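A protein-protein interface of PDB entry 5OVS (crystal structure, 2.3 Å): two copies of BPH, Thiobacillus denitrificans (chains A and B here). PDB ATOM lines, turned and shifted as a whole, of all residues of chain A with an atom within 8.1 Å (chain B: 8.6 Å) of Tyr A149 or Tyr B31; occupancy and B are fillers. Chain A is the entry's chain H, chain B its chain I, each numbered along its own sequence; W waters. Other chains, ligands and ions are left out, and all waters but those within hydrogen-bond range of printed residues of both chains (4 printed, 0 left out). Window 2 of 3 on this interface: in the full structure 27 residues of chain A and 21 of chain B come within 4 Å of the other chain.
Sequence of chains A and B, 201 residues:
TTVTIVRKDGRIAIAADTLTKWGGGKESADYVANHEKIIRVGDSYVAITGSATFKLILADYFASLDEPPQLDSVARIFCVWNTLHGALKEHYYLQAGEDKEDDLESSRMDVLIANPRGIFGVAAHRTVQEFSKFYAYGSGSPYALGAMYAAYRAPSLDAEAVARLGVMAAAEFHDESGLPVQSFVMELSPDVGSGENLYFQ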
ATOM      1  N   ILE A 119     -36.488   2.896  22.069  1.00  0.00           N
ATOM      2  CA  ILE A 119     -35.495   2.589  21.052  1.00  0.00           C
ATOM      3  C   ILE A 119     -34.149   2.314  21.711  1.00  0.00           C
ATOM      4  O   ILE A 119     -33.759   2.972  22.676  1.00  0.00           O
ATOM      5  CB  ILE A 119     -35.381   3.684  19.959  1.00  0.00           C
ATOM      6  CG1 ILE A 119     -35.095   5.063  20.547  1.00  0.00           C
ATOM      7  CG2 ILE A 119     -36.653   3.722  19.141  1.00  0.00           C
ATOM      8  CD1 ILE A 119     -34.556   6.054  19.524  1.00  0.00           C
ATOM      9  N   GLN A 129     -27.388   0.472  24.668  1.00  0.00           N
ATOM     10  CA  GLN A 129     -27.849   1.814  25.007  1.00  0.00           C
ATOM     11  C   GLN A 129     -29.328   1.989  24.684  1.00  0.00           C
ATOM     12  O   GLN A 129     -29.791   1.503  23.658  1.00  0.00           O
ATOM     13  CB  GLN A 129     -27.024   2.835  24.240  1.00  0.00           C
ATOM     14  CG  GLN A 129     -25.594   2.907  24.745  1.00  0.00           C
ATOM     15  CD  GLN A 129     -24.667   3.562  23.749  1.00  0.00           C
ATOM     16  OE1 GLN A 129     -24.710   3.272  22.556  1.00  0.00           O
ATOM     17  NE2 GLN A 129     -23.814   4.440  24.239  1.00  0.00           N
ATOM     18  N   GLU A 130     -30.076   2.652  25.566  1.00  0.00           N
ATOM     19  CA  GLU A 130     -31.377   3.193  25.185  1.00  0.00           C
ATOM     20  C   GLU A 130     -31.140   4.582  24.613  1.00  0.00           C
ATOM     21  O   GLU A 130     -30.395   5.373  25.179  1.00  0.00           O
ATOM     22  CB  GLU A 130     -32.359   3.274  26.358  1.00  0.00           C
ATOM     23  CG  GLU A 130     -33.628   4.061  26.012  1.00  0.00           C
ATOM     24  CD  GLU A 130     -34.844   3.716  26.860  1.00  0.00           C
ATOM     25  OE1 GLU A 130     -34.685   3.053  27.905  1.00  0.00           O
ATOM     26  OE2 GLU A 130     -35.973   4.105  26.473  1.00  0.00           O
ATOM     27  N   PHE A 131     -31.783   4.886  23.497  1.00  0.00           N
ATOM     28  CA  PHE A 131     -31.626   6.190  22.878  1.00  0.00           C
ATOM     29  C   PHE A 131     -32.831   7.063  23.180  1.00  0.00           C
ATOM     30  O   PHE A 131     -33.944   6.556  23.334  1.00  0.00           O
ATOM     31  CB  PHE A 131     -31.416   6.030  21.381  1.00  0.00           C
ATOM     32  CG  PHE A 131     -30.162   5.283  21.037  1.00  0.00           C
ATOM     33  CD1 PHE A 131     -28.912   5.868  21.233  1.00  0.00           C
ATOM     34  CD2 PHE A 131     -30.223   4.004  20.522  1.00  0.00           C
ATOM     35  CE1 PHE A 131     -27.750   5.183  20.913  1.00  0.00           C
ATOM     36  CE2 PHE A 131     -29.073   3.325  20.193  1.00  0.00           C
ATOM     37  CZ  PHE A 131     -27.835   3.910  20.389  1.00  0.00           C
ATOM     38  N   SER A 132     -32.591   8.371  23.286  1.00  0.00           N
ATOM     39  CA  SER A 132     -33.635   9.312  23.663  1.00  0.00           C
ATOM     40  C   SER A 132     -34.191  10.057  22.477  1.00  0.00           C
ATOM     41  O   SER A 132     -35.322  10.517  22.543  1.00  0.00           O
ATOM     42  CB  SER A 132     -33.131  10.312  24.700  1.00  0.00           C
ATOM     43  OG  SER A 132     -32.115  11.128  24.165  1.00  0.00           O
ATOM     44  N   LYS A 133     -33.418  10.179  21.397  1.00  0.00           N
ATOM     45  CA  LYS A 133     -33.866  10.914  20.210  1.00  0.00           C
ATOM     46  C   LYS A 133     -33.752  10.067  18.938  1.00  0.00           C
ATOM     47  O   LYS A 133     -34.757   9.702  18.321  1.00  0.00           O
ATOM     48  CB  LYS A 133     -33.075  12.211  20.063  1.00  0.00           C
ATOM     49  CG  LYS A 133     -33.125  13.117  21.287  1.00  0.00           C
ATOM     50  CD  LYS A 133     -32.202  14.307  21.091  1.00  0.00           C
ATOM     51  CE  LYS A 133     -32.483  15.430  22.077  1.00  0.00           C
ATOM     52  NZ  LYS A 133     -32.348  15.002  23.499  1.00  0.00           N
ATOM     53  N   PHE A 134     -32.529   9.746  18.555  1.00  0.00           N
ATOM     54  CA  PHE A 134     -32.283   8.969  17.346  1.00  0.00           C
ATOM     55  C   PHE A 134     -30.842   8.460  17.337  1.00  0.00           C
ATOM     56  O   PHE A 134     -29.985   8.978  18.066  1.00  0.00           O
ATOM     57  CB  PHE A 134     -32.565   9.802  16.080  1.00  0.00           C
ATOM     58  CG  PHE A 134     -31.707  11.045  15.940  1.00  0.00           C
ATOM     59  CD1 PHE A 134     -30.419  10.969  15.430  1.00  0.00           C
ATOM     60  CD2 PHE A 134     -32.207  12.289  16.275  1.00  0.00           C
ATOM     61  CE1 PHE A 134     -29.640  12.111  15.270  1.00  0.00           C
ATOM     62  CE2 PHE A 134     -31.438  13.437  16.123  1.00  0.00           C
ATOM     63  CZ  PHE A 134     -30.154  13.349  15.621  1.00  0.00           C
ATOM     64  N   TYR A 135     -30.574   7.442  16.529  1.00  0.00           N
ATOM     65  CA  TYR A 135     -29.205   7.004  16.337  1.00  0.00           C
ATOM     66  C   TYR A 135     -29.081   6.227  15.055  1.00  0.00           C
ATOM     67  O   TYR A 135     -30.089   5.955  14.375  1.00  0.00           O
ATOM     68  CB  TYR A 135     -28.678   6.183  17.542  1.00  0.00           C
ATOM     69  CG  TYR A 135     -27.180   6.367  17.743  1.00  0.00           C
ATOM     70  CD1 TYR A 135     -26.634   7.639  17.922  1.00  0.00           C
ATOM     71  CD2 TYR A 135     -26.311   5.279  17.717  1.00  0.00           C
ATOM     72  CE1 TYR A 135     -25.268   7.816  18.072  1.00  0.00           C
ATOM     73  CE2 TYR A 135     -24.942   5.442  17.874  1.00  0.00           C
ATOM     74  CZ  TYR A 135     -24.418   6.708  18.042  1.00  0.00           C
ATOM     75  OH  TYR A 135     -23.044   6.857  18.193  1.00  0.00           O
ATOM     76  N   PRO A 142     -22.331   7.989  10.155  1.00  0.00           N
ATOM     77  CA  PRO A 142     -21.974   9.418  10.261  1.00  0.00           C
ATOM     78  C   PRO A 142     -22.865  10.335   9.398  1.00  0.00           C
ATOM     79  O   PRO A 142     -23.323  11.399   9.848  1.00  0.00           O
ATOM     80  CB  PRO A 142     -20.529   9.453   9.767  1.00  0.00           C
ATOM     81  CG  PRO A 142     -19.996   8.095  10.058  1.00  0.00           C
ATOM     82  CD  PRO A 142     -21.149   7.138   9.932  1.00  0.00           C
ATOM     83  N   TYR A 143     -23.123   9.889   8.179  1.00  0.00           N
ATOM     84  CA  TYR A 143     -23.958  10.616   7.227  1.00  0.00           C
ATOM     85  C   TYR A 143     -25.389  10.725   7.744  1.00  0.00           C
ATOM     86  O   TYR A 143     -26.026  11.772   7.655  1.00  0.00           O
ATOM     87  CB  TYR A 143     -23.977   9.887   5.876  1.00  0.00           C
ATOM     88  CG  TYR A 143     -22.617   9.642   5.284  1.00  0.00           C
ATOM     89  CD1 TYR A 143     -21.898   8.518   5.606  1.00  0.00           C
ATOM     90  CD2 TYR A 143     -22.057  10.536   4.396  1.00  0.00           C
ATOM     91  CE1 TYR A 143     -20.638   8.299   5.075  1.00  0.00           C
ATOM     92  CE2 TYR A 143     -20.809  10.317   3.857  1.00  0.00           C
ATOM     93  CZ  TYR A 143     -20.105   9.198   4.202  1.00  0.00           C
ATOM     94  OH  TYR A 143     -18.862   8.956   3.684  1.00  0.00           O
ATOM     95  N   ALA A 144     -25.871   9.613   8.279  1.00  0.00           N
ATOM     96  CA  ALA A 144     -27.231   9.496   8.746  1.00  0.00           C
ATOM     97  C   ALA A 144     -27.460  10.394   9.943  1.00  0.00           C
ATOM     98  O   ALA A 144     -28.468  11.091  10.014  1.00  0.00           O
ATOM     99  CB  ALA A 144     -27.519   8.050   9.114  1.00  0.00           C
ATOM    100  N   LEU A 145     -26.521  10.348  10.887  1.00  0.00           N
ATOM    101  CA  LEU A 145     -26.604  11.149  12.102  1.00  0.00           C
ATOM    102  C   LEU A 145     -26.604  12.621  11.705  1.00  0.00           C
ATOM    103  O   LEU A 145     -27.413  13.401  12.216  1.00  0.00           O
ATOM    104  CB  LEU A 145     -25.446  10.845  13.059  1.00  0.00           C
ATOM    105  CG  LEU A 145     -25.380   9.482  13.773  1.00  0.00           C
ATOM    106  CD1 LEU A 145     -24.059   9.372  14.522  1.00  0.00           C
ATOM    107  CD2 LEU A 145     -26.540   9.228  14.732  1.00  0.00           C
ATOM    108  N   GLY A 146     -25.705  12.991  10.790  1.00  0.00           N
ATOM    109  CA  GLY A 146     -25.680  14.345  10.247  1.00  0.00           C
ATOM    110  C   GLY A 146     -27.044  14.783   9.745  1.00  0.00           C
ATOM    111  O   GLY A 146     -27.632  15.760  10.232  1.00  0.00           O
ATOM    112  N   ALA A 147     -27.554  14.038   8.773  1.00  0.00           N
ATOM    113  CA  ALA A 147     -28.856  14.319   8.185  1.00  0.00           C
ATOM    114  C   ALA A 147     -29.955  14.460   9.234  1.00  0.00           C
ATOM    115  O   ALA A 147     -30.647  15.478   9.276  1.00  0.00           O
ATOM    116  CB  ALA A 147     -29.209  13.226   7.198  1.00  0.00           C
ATOM    117  N   MET A 148     -30.087  13.439  10.086  1.00  0.00           N
ATOM    118  CA  MET A 148     -31.131  13.370  11.098  1.00  0.00           C
ATOM    119  C   MET A 148     -31.026  14.475  12.157  1.00  0.00           C
ATOM    120  O   MET A 148     -32.036  14.975  12.636  1.00  0.00           O
ATOM    121  CB  MET A 148     -31.098  12.001  11.783  1.00  0.00           C
ATOM    122  CG  MET A 148     -31.399  10.836  10.854  1.00  0.00           C
ATOM    123  SD  MET A 148     -31.811   9.365  11.800  1.00  0.00           S
ATOM    124  CE  MET A 148     -30.220   8.912  12.504  1.00  0.00           C
ATOM    125  N   TYR A 149     -29.812  14.844  12.539  1.00  0.00           N
ATOM    126  CA  TYR A 149     -29.601  16.061  13.335  1.00  0.00           C
ATOM    127  C   TYR A 149     -30.261  17.308  12.710  1.00  0.00           C
ATOM    128  O   TYR A 149     -30.850  18.127  13.414  1.00  0.00           O
ATOM    129  CB  TYR A 149     -28.101  16.312  13.484  1.00  0.00           C
ATOM    130  CG  TYR A 149     -27.727  17.602  14.170  1.00  0.00           C
ATOM    131  CD1 TYR A 149     -27.734  17.695  15.560  1.00  0.00           C
ATOM    132  CD2 TYR A 149     -27.332  18.709  13.437  1.00  0.00           C
ATOM    133  CE1 TYR A 149     -27.385  18.870  16.200  1.00  0.00           C
ATOM    134  CE2 TYR A 149     -26.985  19.889  14.071  1.00  0.00           C
ATOM    135  CZ  TYR A 149     -27.015  19.965  15.449  1.00  0.00           C
ATOM    136  OH  TYR A 149     -26.678  21.128  16.094  1.00  0.00           O
ATOM    137  N   ALA A 150     -30.138  17.447  11.394  1.00  0.00           N
ATOM    138  CA  ALA A 150     -30.633  18.627  10.698  1.00  0.00           C
ATOM    139  C   ALA A 150     -32.135  18.579  10.432  1.00  0.00           C
ATOM    140  O   ALA A 150     -32.703  19.576  10.020  1.00  0.00           O
ATOM    141  CB  ALA A 150     -29.892  18.804   9.387  1.00  0.00           C
ATOM    142  N   ALA A 151     -32.770  17.430  10.643  1.00  0.00           N
ATOM    143  CA  ALA A 151     -34.191  17.268  10.320  1.00  0.00           C
ATOM    144  C   ALA A 151     -35.069  16.869  11.514  1.00  0.00           C
ATOM    145  O   ALA A 151     -36.302  16.910  11.427  1.00  0.00           O
ATOM    146  CB  ALA A 151     -34.348  16.247   9.204  1.00  0.00           C
ATOM    147  N   TYR A 152     -34.456  16.505  12.628  1.00  0.00           N
ATOM    148  CA  TYR A 152     -35.201  15.943  13.733  1.00  0.00           C
ATOM    149  C   TYR A 152     -36.363  16.817  14.192  1.00  0.00           C
ATOM    150  O   TYR A 152     -37.427  16.304  14.524  1.00  0.00           O
ATOM    151  CB  TYR A 152     -34.286  15.716  14.921  1.00  0.00           C
ATOM    152  CG  TYR A 152     -34.959  14.974  16.043  1.00  0.00           C
ATOM    153  CD1 TYR A 152     -35.576  13.747  15.819  1.00  0.00           C
ATOM    154  CD2 TYR A 152     -34.981  15.492  17.327  1.00  0.00           C
ATOM    155  CE1 TYR A 152     -36.192  13.051  16.847  1.00  0.00           C
ATOM    156  CE2 TYR A 152     -35.592  14.804  18.365  1.00  0.00           C
ATOM    157  CZ  TYR A 152     -36.190  13.586  18.116  1.00  0.00           C
ATOM    158  OH  TYR A 152     -36.793  12.912  19.138  1.00  0.00           O
ATOM    159  N   ARG A 153     -36.153  18.127  14.211  1.00  0.00           N
ATOM    160  CA  ARG A 153     -37.121  19.045  14.795  1.00  0.00           C
ATOM    161  C   ARG A 153     -38.068  19.681  13.763  1.00  0.00           C
ATOM    162  O   ARG A 153     -38.909  20.504  14.122  1.00  0.00           O
ATOM    163  CB  ARG A 153     -36.383  20.122  15.608  1.00  0.00           C
ATOM    164  CG  ARG A 153     -35.254  19.556  16.463  1.00  0.00           C
ATOM    165  CD  ARG A 153     -34.818  20.471  17.599  1.00  0.00           C
ATOM    166  NE  ARG A 153     -35.065  19.863  18.914  1.00  0.00           N
ATOM    167  CZ  ARG A 153     -34.317  18.907  19.475  1.00  0.00           C
ATOM    168  NH1 ARG A 153     -33.249  18.416  18.849  1.00  0.00           N
ATOM    169  NH2 ARG A 153     -34.636  18.429  20.675  1.00  0.00           N
ATOM    170  N   ALA A 154     -37.948  19.298  12.493  1.00  0.00           N
ATOM    171  CA  ALA A 154     -38.852  19.809  11.466  1.00  0.00           C
ATOM    172  C   ALA A 154     -40.238  19.216  11.704  1.00  0.00           C
ATOM    173  O   ALA A 154     -40.374  17.990  11.757  1.00  0.00           O
ATOM    174  CB  ALA A 154     -38.355  19.453  10.073  1.00  0.00           C
ATOM    175  N   VAL A 162     -37.873  10.914   9.211  1.00  0.00           N
ATOM    176  CA  VAL A 162     -36.517  11.264   9.667  1.00  0.00           C
ATOM    177  C   VAL A 162     -35.581  10.065   9.570  1.00  0.00           C
ATOM    178  O   VAL A 162     -34.499  10.174   9.002  1.00  0.00           O
ATOM    179  CB  VAL A 162     -36.496  11.807  11.119  1.00  0.00           C
ATOM    180  CG1 VAL A 162     -35.066  11.993  11.617  1.00  0.00           C
ATOM    181  CG2 VAL A 162     -37.239  13.130  11.219  1.00  0.00           C
ATOM    182  N   LEU A 165     -34.775   9.541   5.961  1.00  0.00           N
ATOM    183  CA  LEU A 165     -33.850  10.567   5.475  1.00  0.00           C
ATOM    184  C   LEU A 165     -32.414  10.242   5.882  1.00  0.00           C
ATOM    185  O   LEU A 165     -31.454  10.622   5.189  1.00  0.00           O
ATOM    186  CB  LEU A 165     -34.230  11.922   6.043  1.00  0.00           C
ATOM    187  CG  LEU A 165     -33.465  13.128   5.510  1.00  0.00           C
ATOM    188  CD1 LEU A 165     -33.662  13.289   4.006  1.00  0.00           C
ATOM    189  CD2 LEU A 165     -33.948  14.359   6.255  1.00  0.00           C
ATOM    190  N   GLY A 166     -32.276   9.557   7.021  1.00  0.00           N
ATOM    191  CA  GLY A 166     -30.974   9.188   7.543  1.00  0.00           C
ATOM    192  C   GLY A 166     -30.290   8.249   6.579  1.00  0.00           C
ATOM    193  O   GLY A 166     -29.152   8.479   6.173  1.00  0.00           O
ATOM    194  N   THR B  18     -20.513  11.677  31.692  1.00  0.00           N
ATOM    195  CA  THR B  18     -21.629  10.899  31.148  1.00  0.00           C
ATOM    196  C   THR B  18     -21.488  10.585  29.671  1.00  0.00           C
ATOM    197  O   THR B  18     -22.418  10.058  29.060  1.00  0.00           O
ATOM    198  CB  THR B  18     -22.953  11.655  31.345  1.00  0.00           C
ATOM    199  OG1 THR B  18     -22.787  13.019  30.944  1.00  0.00           O
ATOM    200  CG2 THR B  18     -23.378  11.611  32.812  1.00  0.00           C
ATOM    201  N   LEU B  19     -20.328  10.913  29.099  1.00  0.00           N
ATOM    202  CA  LEU B  19     -20.095  10.797  27.667  1.00  0.00           C
ATOM    203  C   LEU B  19     -19.565   9.417  27.315  1.00  0.00           C
ATOM    204  O   LEU B  19     -18.629   8.937  27.943  1.00  0.00           O
ATOM    205  CB  LEU B  19     -19.061  11.831  27.216  1.00  0.00           C
ATOM    206  CG  LEU B  19     -18.633  11.752  25.754  1.00  0.00           C
ATOM    207  CD1 LEU B  19     -19.805  12.047  24.843  1.00  0.00           C
ATOM    208  CD2 LEU B  19     -17.511  12.739  25.507  1.00  0.00           C
ATOM    209  N   LYS B  26     -19.037  10.749  19.453  1.00  0.00           N
ATOM    210  CA  LYS B  26     -19.522  11.127  20.765  1.00  0.00           C
ATOM    211  C   LYS B  26     -20.969  10.682  20.901  1.00  0.00           C
ATOM    212  O   LYS B  26     -21.767  10.840  19.979  1.00  0.00           O
ATOM    213  CB  LYS B  26     -19.459  12.640  20.947  1.00  0.00           C
ATOM    214  CG  LYS B  26     -18.054  13.210  20.890  1.00  0.00           C
ATOM    215  CD  LYS B  26     -18.021  14.697  21.223  1.00  0.00           C
ATOM    216  CE  LYS B  26     -18.725  15.540  20.184  1.00  0.00           C
ATOM    217  NZ  LYS B  26     -18.606  16.986  20.505  1.00  0.00           N
ATOM    218  N   GLU B  27     -21.273  10.107  22.061  1.00  0.00           N
ATOM    219  CA  GLU B  27     -22.607   9.694  22.430  1.00  0.00           C
ATOM    220  C   GLU B  27     -22.897  10.327  23.801  1.00  0.00           C
ATOM    221  O   GLU B  27     -22.654   9.731  24.849  1.00  0.00           O
ATOM    222  CB  GLU B  27     -22.669   8.169  22.458  1.00  0.00           C
ATOM    223  CG  GLU B  27     -22.293   7.559  21.112  1.00  0.00           C
ATOM    224  CD  GLU B  27     -22.167   6.037  21.104  1.00  0.00           C
ATOM    225  OE1 GLU B  27     -21.894   5.438  22.161  1.00  0.00           O
ATOM    226  OE2 GLU B  27     -22.312   5.433  20.016  1.00  0.00           O
ATOM    227  N   SER B  28     -23.383  11.561  23.792  1.00  0.00           N
ATOM    228  CA  SER B  28     -23.565  12.303  25.045  1.00  0.00           C
ATOM    229  C   SER B  28     -24.837  11.872  25.762  1.00  0.00           C
ATOM    230  O   SER B  28     -25.665  11.152  25.197  1.00  0.00           O
ATOM    231  CB  SER B  28     -23.643  13.791  24.775  1.00  0.00           C
ATOM    232  OG  SER B  28     -24.851  14.068  24.112  1.00  0.00           O
ATOM    233  N   ALA B  29     -25.001  12.349  26.998  1.00  0.00           N
ATOM    234  CA  ALA B  29     -26.193  12.055  27.783  1.00  0.00           C
ATOM    235  C   ALA B  29     -27.425  12.574  27.078  1.00  0.00           C
ATOM    236  O   ALA B  29     -28.521  12.123  27.362  1.00  0.00           O
ATOM    237  CB  ALA B  29     -26.093  12.667  29.166  1.00  0.00           C
ATOM    238  N   ASP B  30     -27.239  13.524  26.159  1.00  0.00           N
ATOM    239  CA  ASP B  30     -28.353  14.097  25.418  1.00  0.00           C
ATOM    240  C   ASP B  30     -28.961  13.142  24.388  1.00  0.00           C
ATOM    241  O   ASP B  30     -30.104  13.316  23.984  1.00  0.00           O
ATOM    242  CB  ASP B  30     -27.925  15.392  24.720  1.00  0.00           C
ATOM    243  CG  ASP B  30     -29.102  16.296  24.410  1.00  0.00           C
ATOM    244  OD1 ASP B  30     -30.156  16.133  25.068  1.00  0.00           O
ATOM    245  OD2 ASP B  30     -28.972  17.162  23.518  1.00  0.00           O
ATOM    246  N   TYR B  31     -28.188  12.157  23.944  1.00  0.00           N
ATOM    247  CA  TYR B  31     -28.678  11.139  23.015  1.00  0.00           C
ATOM    248  C   TYR B  31     -28.844   9.775  23.683  1.00  0.00           C
ATOM    249  O   TYR B  31     -29.610   8.944  23.200  1.00  0.00           O
ATOM    250  CB  TYR B  31     -27.749  11.034  21.818  1.00  0.00           C
ATOM    251  CG  TYR B  31     -27.786  12.255  20.936  1.00  0.00           C
ATOM    252  CD1 TYR B  31     -27.044  13.380  21.231  1.00  0.00           C
ATOM    253  CD2 TYR B  31     -28.573  12.282  19.805  1.00  0.00           C
ATOM    254  CE1 TYR B  31     -27.083  14.506  20.416  1.00  0.00           C
ATOM    255  CE2 TYR B  31     -28.623  13.403  18.993  1.00  0.00           C
ATOM    256  CZ  TYR B  31     -27.878  14.512  19.299  1.00  0.00           C
ATOM    257  OH  TYR B  31     -27.952  15.611  18.471  1.00  0.00           O
ATOM    258  N   VAL B  32     -28.156   9.552  24.796  1.00  0.00           N
ATOM    259  CA  VAL B  32     -28.179   8.247  25.445  1.00  0.00           C
ATOM    260  C   VAL B  32     -28.853   8.337  26.806  1.00  0.00           C
ATOM    261  O   VAL B  32     -28.445   9.109  27.665  1.00  0.00           O
ATOM    262  CB  VAL B  32     -26.759   7.665  25.599  1.00  0.00           C
ATOM    263  CG1 VAL B  32     -26.798   6.316  26.315  1.00  0.00           C
ATOM    264  CG2 VAL B  32     -26.102   7.517  24.238  1.00  0.00           C
ATOM    265  N   ALA B  33     -29.880   7.524  26.995  1.00  0.00           N
ATOM    266  CA  ALA B  33     -30.672   7.578  28.205  1.00  0.00           C
ATOM    267  C   ALA B  33     -29.937   6.989  29.393  1.00  0.00           C
ATOM    268  O   ALA B  33     -30.012   7.519  30.496  1.00  0.00           O
ATOM    269  CB  ALA B  33     -31.987   6.855  27.995  1.00  0.00           C
ATOM    270  N   ASN B  34     -29.225   5.891  29.162  1.00  0.00           N
ATOM    271  CA  ASN B  34     -28.545   5.176  30.234  1.00  0.00           C
ATOM    272  C   ASN B  34     -27.076   5.567  30.306  1.00  0.00           C
ATOM    273  O   ASN B  34     -26.192   4.731  30.182  1.00  0.00           O
ATOM    274  CB  ASN B  34     -28.727   3.656  30.069  1.00  0.00           C
ATOM    275  CG  ASN B  34     -28.192   3.126  28.741  1.00  0.00           C
ATOM    276  OD1 ASN B  34     -28.489   3.663  27.672  1.00  0.00           O
ATOM    277  ND2 ASN B  34     -27.405   2.055  28.808  1.00  0.00           N
ATOM    278  N   HIS B  35     -26.837   6.852  30.550  1.00  0.00           N
ATOM    279  CA  HIS B  35     -25.513   7.470  30.392  1.00  0.00           C
ATOM    280  C   HIS B  35     -24.725   7.537  31.701  1.00  0.00           C
ATOM    281  O   HIS B  35     -23.605   8.059  31.724  1.00  0.00           O
ATOM    282  CB  HIS B  35     -25.663   8.881  29.809  1.00  0.00           C
ATOM    283  CG  HIS B  35     -26.680   9.715  30.511  1.00  0.00           C
ATOM    284  ND1 HIS B  35     -27.945   9.923  30.007  1.00  0.00           N
ATOM    285  CD2 HIS B  35     -26.635  10.372  31.695  1.00  0.00           C
ATOM    286  CE1 HIS B  35     -28.635  10.679  30.844  1.00  0.00           C
ATOM    287  NE2 HIS B  35     -27.861  10.968  31.876  1.00  0.00           N
ATOM    288  N   PRO B 180     -23.188  16.294  31.001  1.00  0.00           N
ATOM    289  CA  PRO B 180     -23.184  16.590  32.443  1.00  0.00           C
ATOM    290  C   PRO B 180     -22.328  15.673  33.325  1.00  0.00           C
ATOM    291  O   PRO B 180     -21.946  14.563  32.926  1.00  0.00           O
ATOM    292  CB  PRO B 180     -24.665  16.482  32.834  1.00  0.00           C
ATOM    293  CG  PRO B 180     -25.296  15.643  31.778  1.00  0.00           C
ATOM    294  CD  PRO B 180     -24.520  15.881  30.521  1.00  0.00           C
HETATM  295  O   HOH W   1     -31.143  16.960  18.794  1.00  0.00           O
HETATM  296  O   HOH W   2     -31.034  11.660  26.575  1.00  0.00           O
HETATM  297  O   HOH W   3     -30.662   9.605  20.653  1.00  0.00           O
HETATM  298  O   HOH W   4     -21.501   9.017  17.852  1.00  0.00           O
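The backbone carbonyl oxygen (O) of Ile A119 is in hydrogen-bond range of the backbone NH (N) of Phe A131 (2.9 Å).
OG of Ser B28 sits close to N of Asp B30.
ND1 of His B35 lies within hydrogen-bond range of O of Val B32 (2.5 Å).
O of Ala B33 lies within hydrogen-bond range of ND1 of His B35, 3.2 Å away.
OE1 of Glu B27 sits at hydrogen-bond distance from NE2 of Gln A129.
The backbone carbonyl oxygen (O) of Glu A130 lies within hydrogen-bond range of the backbone NH (N) of Ala B33, at 2.9 Å.
N of Glu A130 is in hydrogen-bond range of OD1 of Asn B34 (2.8 Å).
The side-chain hydroxyl of Ser A132 lies within hydrogen-bond range of the backbone carbonyl oxygen of Asp B30 (3.0 Å).
N of Ser A132 lies within hydrogen-bond range of O of Tyr B31.
The side-chain carboxylate (OD1) of Asp B30 is in salt-bridge range of the side-chain amino group (NZ) of Lys A133 (2.9 Å).
OE2 of Glu B27 lies within hydrogen-bond range of OH of Tyr A135 (2.4 Å).
Water W1 lies within hydrogen-bond range of NH1 of Arg A153 and OH of Tyr B31.
Water W2 lies within hydrogen-bond range of O of Ala B29 (2.7 Å), OG of Ser A132 (2.7 Å) and O of Asp B30 (3.2 Å).
Water W4 lies within hydrogen-bond range of OH of Tyr A135 and O of Lys B26.
Water W3 lies within hydrogen-bond range of the backbone carbonyl oxygen (O) of Phe A134 (2.7 Å), the backbone carbonyl oxygen (O) of Tyr B31 (2.8 Å), the backbone NH (N) of Lys A133 (2.9 Å) and the backbone NH (N) of Ser A132 (3.5 Å).
Among the printed residues, pairs that only touch across the chains: Gln A129 with Asn B34, Phe A131 with Tyr B31, Tyr A149 with Tyr B31, Glu A130 with Val B32, Phe A134 with Tyr B31 and Gln A129 with Val B32.
Of the printed residues of chain B, Glu A130 touches Val B32, Ala B33 and Asn B34.
Of the printed residues of chain B, Lys A133 touches Asp B30 (2.8 Å).
No residue of chain B comes within 4 Å of Ala A150.
Tyr A152 touches none of the printed residues of chain B.
Leu B19 touches none of the printed residues of chain A.
The nearest residue of chain A that does not touch Tyr B31 is Glu A130 (4.2 Å).
The nearest printed residue of chain A that does not touch Asp B30 is Arg A153 (6.5 Å).
Of the 24 printed residues of chain A, 8 touch a printed residue of chain B.
Printed residues of chain A that touch a printed residue of chain B: Gln A129, Glu A130, Phe A131, Ser A132, Lys A133, Phe A134, Tyr A135 and Tyr A149.
Hydrophobic or aromatic side chains of chain A within 4 Å of the printed part of chain B: Phe A131, Phe A134, Tyr A135 and Tyr A149.
No position is printed for both chains.
Of the 13 pairs that touch across the chains among the printed residues, none has its exchanged pair printed and touching as well.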
